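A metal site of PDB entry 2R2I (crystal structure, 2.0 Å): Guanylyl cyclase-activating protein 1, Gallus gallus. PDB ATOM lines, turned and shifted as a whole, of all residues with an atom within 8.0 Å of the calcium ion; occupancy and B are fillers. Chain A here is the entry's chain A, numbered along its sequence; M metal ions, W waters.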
ATOM      1  N   PHE A  94     -36.355  -9.968 -14.411  1.00  0.00           N
ATOM      2  CA  PHE A  94     -34.952  -9.699 -14.056  1.00  0.00           C
ATOM      3  C   PHE A  94     -34.031 -10.295 -15.112  1.00  0.00           C
ATOM      4  O   PHE A  94     -33.102  -9.625 -15.585  1.00  0.00           O
ATOM      5  CB  PHE A  94     -34.616 -10.282 -12.683  1.00  0.00           C
ATOM      6  CG  PHE A  94     -33.191 -10.033 -12.256  1.00  0.00           C
ATOM      7  CD1 PHE A  94     -32.153 -10.832 -12.711  1.00  0.00           C
ATOM      8  CD2 PHE A  94     -32.884  -8.957 -11.421  1.00  0.00           C
ATOM      9  CE1 PHE A  94     -30.833 -10.568 -12.362  1.00  0.00           C
ATOM     10  CE2 PHE A  94     -31.569  -8.685 -11.060  1.00  0.00           C
ATOM     11  CZ  PHE A  94     -30.546  -9.480 -11.535  1.00  0.00           C
ATOM     12  N   LYS A  95     -34.276 -11.539 -15.485  1.00  0.00           N
ATOM     13  CA  LYS A  95     -33.456 -12.216 -16.484  1.00  0.00           C
ATOM     14  C   LYS A  95     -33.526 -11.497 -17.816  1.00  0.00           C
ATOM     15  O   LYS A  95     -32.557 -11.499 -18.583  1.00  0.00           O
ATOM     16  CB  LYS A  95     -33.903 -13.668 -16.660  1.00  0.00           C
ATOM     17  CG  LYS A  95     -33.755 -14.517 -15.400  1.00  0.00           C
ATOM     18  CD  LYS A  95     -34.083 -15.977 -15.670  1.00  0.00           C
ATOM     19  CE  LYS A  95     -33.079 -16.596 -16.633  1.00  0.00           C
ATOM     20  NZ  LYS A  95     -33.464 -17.996 -17.003  1.00  0.00           N
ATOM     21  N   TYR A  97     -34.004  -8.162 -18.218  1.00  0.00           N
ATOM     22  CA  TYR A  97     -33.226  -6.934 -18.072  1.00  0.00           C
ATOM     23  C   TYR A  97     -31.721  -7.218 -18.067  1.00  0.00           C
ATOM     24  O   TYR A  97     -30.936  -6.381 -18.515  1.00  0.00           O
ATOM     25  CB  TYR A  97     -33.611  -6.200 -16.781  1.00  0.00           C
ATOM     26  CG  TYR A  97     -35.001  -5.630 -16.806  1.00  0.00           C
ATOM     27  CD1 TYR A  97     -35.414  -4.797 -17.848  1.00  0.00           C
ATOM     28  CD2 TYR A  97     -35.924  -5.941 -15.804  1.00  0.00           C
ATOM     29  CE1 TYR A  97     -36.709  -4.279 -17.895  1.00  0.00           C
ATOM     30  CE2 TYR A  97     -37.217  -5.427 -15.837  1.00  0.00           C
ATOM     31  CZ  TYR A  97     -37.604  -4.607 -16.886  1.00  0.00           C
ATOM     32  OH  TYR A  97     -38.887  -4.113 -16.927  1.00  0.00           O
ATOM     33  N   ASP A  98     -31.329  -8.381 -17.537  1.00  0.00           N
ATOM     34  CA  ASP A  98     -29.930  -8.776 -17.483  1.00  0.00           C
ATOM     35  C   ASP A  98     -29.500  -9.224 -18.881  1.00  0.00           C
ATOM     36  O   ASP A  98     -29.379 -10.421 -19.157  1.00  0.00           O
ATOM     37  CB  ASP A  98     -29.737  -9.916 -16.479  1.00  0.00           C
ATOM     38  CG  ASP A  98     -28.284 -10.376 -16.370  1.00  0.00           C
ATOM     39  OD1 ASP A  98     -27.373  -9.649 -16.839  1.00  0.00           O
ATOM     40  OD2 ASP A  98     -28.050 -11.466 -15.797  1.00  0.00           O
ATOM     41  N   VAL A  99     -29.252  -8.261 -19.760  1.00  0.00           N
ATOM     42  CA  VAL A  99     -28.878  -8.546 -21.139  1.00  0.00           C
ATOM     43  C   VAL A  99     -27.700  -9.518 -21.331  1.00  0.00           C
ATOM     44  O   VAL A  99     -27.807 -10.467 -22.111  1.00  0.00           O
ATOM     45  CB  VAL A  99     -28.588  -7.227 -21.926  1.00  0.00           C
ATOM     46  CG1 VAL A  99     -28.394  -7.513 -23.422  1.00  0.00           C
ATOM     47  CG2 VAL A  99     -29.745  -6.258 -21.731  1.00  0.00           C
ATOM     48  N   ASP A 100     -26.601  -9.310 -20.617  1.00  0.00           N
ATOM     49  CA  ASP A 100     -25.451 -10.181 -20.797  1.00  0.00           C
ATOM     50  C   ASP A 100     -25.466 -11.441 -19.934  1.00  0.00           C
ATOM     51  O   ASP A 100     -24.540 -12.255 -19.992  1.00  0.00           O
ATOM     52  CB  ASP A 100     -24.138  -9.399 -20.598  1.00  0.00           C
ATOM     53  CG  ASP A 100     -23.845  -9.067 -19.141  1.00  0.00           C
ATOM     54  OD1 ASP A 100     -24.726  -9.207 -18.272  1.00  0.00           O
ATOM     55  OD2 ASP A 100     -22.698  -8.661 -18.874  1.00  0.00           O
ATOM     56  N   GLY A 101     -26.526 -11.599 -19.150  1.00  0.00           N
ATOM     57  CA  GLY A 101     -26.674 -12.783 -18.321  1.00  0.00           C
ATOM     58  C   GLY A 101     -25.594 -13.026 -17.292  1.00  0.00           C
ATOM     59  O   GLY A 101     -25.288 -14.178 -16.970  1.00  0.00           O
ATOM     60  N   ASN A 102     -25.002 -11.955 -16.773  1.00  0.00           N
ATOM     61  CA  ASN A 102     -23.957 -12.108 -15.773  1.00  0.00           C
ATOM     62  C   ASN A 102     -24.573 -12.143 -14.365  1.00  0.00           C
ATOM     63  O   ASN A 102     -23.852 -12.134 -13.369  1.00  0.00           O
ATOM     64  CB  ASN A 102     -22.911 -10.979 -15.887  1.00  0.00           C
ATOM     65  CG  ASN A 102     -23.374  -9.658 -15.289  1.00  0.00           C
ATOM     66  OD1 ASN A 102     -24.566  -9.372 -15.232  1.00  0.00           O
ATOM     67  ND2 ASN A 102     -22.412  -8.843 -14.852  1.00  0.00           N
ATOM     68  N   GLY A 103     -25.906 -12.180 -14.319  1.00  0.00           N
ATOM     69  CA  GLY A 103     -26.616 -12.240 -13.048  1.00  0.00           C
ATOM     70  C   GLY A 103     -26.881 -10.902 -12.375  1.00  0.00           C
ATOM     71  O   GLY A 103     -27.376 -10.856 -11.244  1.00  0.00           O
ATOM     72  N   CYS A 104     -26.588  -9.823 -13.077  1.00  0.00           N
ATOM     73  CA  CYS A 104     -26.787  -8.477 -12.553  1.00  0.00           C
ATOM     74  C   CYS A 104     -27.355  -7.551 -13.613  1.00  0.00           C
ATOM     75  O   CYS A 104     -27.037  -7.680 -14.797  1.00  0.00           O
ATOM     76  CB  CYS A 104     -25.441  -7.914 -12.074  1.00  0.00           C
ATOM     77  SG  CYS A 104     -24.497  -9.039 -11.006  1.00  0.00           S
ATOM     78  N   ILE A 105     -28.190  -6.604 -13.201  1.00  0.00           N
ATOM     79  CA  ILE A 105     -28.750  -5.636 -14.138  1.00  0.00           C
ATOM     80  C   ILE A 105     -27.995  -4.318 -13.978  1.00  0.00           C
ATOM     81  O   ILE A 105     -28.085  -3.683 -12.936  1.00  0.00           O
ATOM     82  CB  ILE A 105     -30.243  -5.325 -13.854  1.00  0.00           C
ATOM     83  CG1 ILE A 105     -31.085  -6.595 -13.959  1.00  0.00           C
ATOM     84  CG2 ILE A 105     -30.742  -4.264 -14.846  1.00  0.00           C
ATOM     85  CD1 ILE A 105     -32.539  -6.397 -13.550  1.00  0.00           C
ATOM     86  N   ASP A 106     -27.236  -3.909 -14.996  1.00  0.00           N
ATOM     87  CA  ASP A 106     -26.547  -2.636 -14.876  1.00  0.00           C
ATOM     88  C   ASP A 106     -27.417  -1.545 -15.496  1.00  0.00           C
ATOM     89  O   ASP A 106     -28.394  -1.822 -16.187  1.00  0.00           O
ATOM     90  CB  ASP A 106     -25.144  -2.668 -15.541  1.00  0.00           C
ATOM     91  CG  ASP A 106     -25.177  -2.873 -17.049  1.00  0.00           C
ATOM     92  OD1 ASP A 106     -25.793  -2.055 -17.770  1.00  0.00           O
ATOM     93  OD2 ASP A 106     -24.581  -3.862 -17.514  1.00  0.00           O
ATOM     94  N   ARG A 107     -27.056  -0.305 -15.192  1.00  0.00           N
ATOM     95  CA  ARG A 107     -27.730   0.902 -15.663  1.00  0.00           C
ATOM     96  C   ARG A 107     -27.991   0.876 -17.182  1.00  0.00           C
ATOM     97  O   ARG A 107     -29.113   1.126 -17.637  1.00  0.00           O
ATOM     98  CB  ARG A 107     -26.831   2.092 -15.300  1.00  0.00           C
ATOM     99  CG  ARG A 107     -27.326   3.484 -15.599  1.00  0.00           C
ATOM    100  CD  ARG A 107     -26.095   4.403 -15.637  1.00  0.00           C
ATOM    101  NE  ARG A 107     -26.424   5.808 -15.435  1.00  0.00           N
ATOM    102  CZ  ARG A 107     -25.574   6.806 -15.628  1.00  0.00           C
ATOM    103  NH1 ARG A 107     -24.338   6.562 -16.050  1.00  0.00           N
ATOM    104  NH2 ARG A 107     -25.960   8.047 -15.399  1.00  0.00           N
ATOM    105  N   GLU A 109     -28.002  -1.729 -19.287  1.00  0.00           N
ATOM    106  CA  GLU A 109     -28.912  -2.813 -19.662  1.00  0.00           C
ATOM    107  C   GLU A 109     -30.368  -2.437 -19.393  1.00  0.00           C
ATOM    108  O   GLU A 109     -31.227  -2.596 -20.267  1.00  0.00           O
ATOM    109  CB  GLU A 109     -28.569  -4.089 -18.875  1.00  0.00           C
ATOM    110  CG  GLU A 109     -27.217  -4.695 -19.257  1.00  0.00           C
ATOM    111  CD  GLU A 109     -26.862  -5.921 -18.428  1.00  0.00           C
ATOM    112  OE1 GLU A 109     -27.196  -5.935 -17.225  1.00  0.00           O
ATOM    113  OE2 GLU A 109     -26.234  -6.845 -18.968  1.00  0.00           O
ATOM    114  N   LEU A 110     -30.640  -1.920 -18.197  1.00  0.00           N
ATOM    115  CA  LEU A 110     -31.995  -1.527 -17.841  1.00  0.00           C
ATOM    116  C   LEU A 110     -32.532  -0.456 -18.780  1.00  0.00           C
ATOM    117  O   LEU A 110     -33.693  -0.512 -19.194  1.00  0.00           O
ATOM    118  CB  LEU A 110     -32.053  -1.016 -16.394  1.00  0.00           C
ATOM    119  CG  LEU A 110     -33.442  -0.613 -15.888  1.00  0.00           C
ATOM    120  CD1 LEU A 110     -34.343  -1.837 -15.912  1.00  0.00           C
ATOM    121  CD2 LEU A 110     -33.351  -0.049 -14.483  1.00  0.00           C
ATOM    122  N   GLU A 147     -25.059  -1.818 -10.106  1.00  0.00           N
ATOM    123  CA  GLU A 147     -25.611  -3.088 -10.556  1.00  0.00           C
ATOM    124  C   GLU A 147     -26.782  -3.458  -9.656  1.00  0.00           C
ATOM    125  O   GLU A 147     -26.785  -3.137  -8.474  1.00  0.00           O
ATOM    126  CB  GLU A 147     -24.557  -4.194 -10.443  1.00  0.00           C
ATOM    127  CG  GLU A 147     -23.261  -3.929 -11.169  1.00  0.00           C
ATOM    128  CD  GLU A 147     -22.217  -4.989 -10.839  1.00  0.00           C
ATOM    129  OE1 GLU A 147     -21.421  -4.788  -9.893  1.00  0.00           O
ATOM    130  OE2 GLU A 147     -22.229  -6.034 -11.520  1.00  0.00           O
ATOM    131  N   LEU A 148     -27.772  -4.131 -10.225  1.00  0.00           N
ATOM    132  CA  LEU A 148     -28.923  -4.583  -9.441  1.00  0.00           C
ATOM    133  C   LEU A 148     -28.853  -6.105  -9.315  1.00  0.00           C
ATOM    134  O   LEU A 148     -28.892  -6.818 -10.325  1.00  0.00           O
ATOM    135  CB  LEU A 148     -30.239  -4.208 -10.107  1.00  0.00           C
ATOM    136  CG  LEU A 148     -30.552  -2.741 -10.365  1.00  0.00           C
ATOM    137  CD1 LEU A 148     -31.939  -2.639 -10.954  1.00  0.00           C
ATOM    138  CD2 LEU A 148     -30.452  -1.945  -9.070  1.00  0.00           C
HETATM  139 CA    CA M   1     -25.916  -7.953 -16.700  1.00  0.00          CA
HETATM  140  O   HOH W   1     -24.331  -6.151 -16.026  1.00  0.00           O
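OD2 of Asp 98 lies within hydrogen-bond range of N of Gly 103 (2.7 Å).
The side-chain carboxylate (OE2) of Glu 109 lies close to the backbone NH (N) of Val 99 (3.4 Å).
N of Glu 109 sits at hydrogen-bond distance from OD1 of Asp 106, 2.7 Å away.
N of Gly 101 lies close to OD1 of Asp 98 (3.1 Å).
Within 4 Å of the calcium ion: Asp 98, Asp 100, Asn 102, Cys 104 and Glu 109.
The nearest printed residue that does not touch the calcium ion is Asp 106 (4.4 Å).
The calcium ion is bound by O of Cys 104 (2.2 Å), OD1 of Asp 98 (2.2 Å), OD1 of Asp 100 (2.3 Å), OE1 of Glu 109 (2.4 Å), OD1 of Asn 102 (2.4 Å), water W1 (2.5 Å) and OE2 of Glu 109 (2.5 Å).
The calcium ion has seven donor atoms within binding distance.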
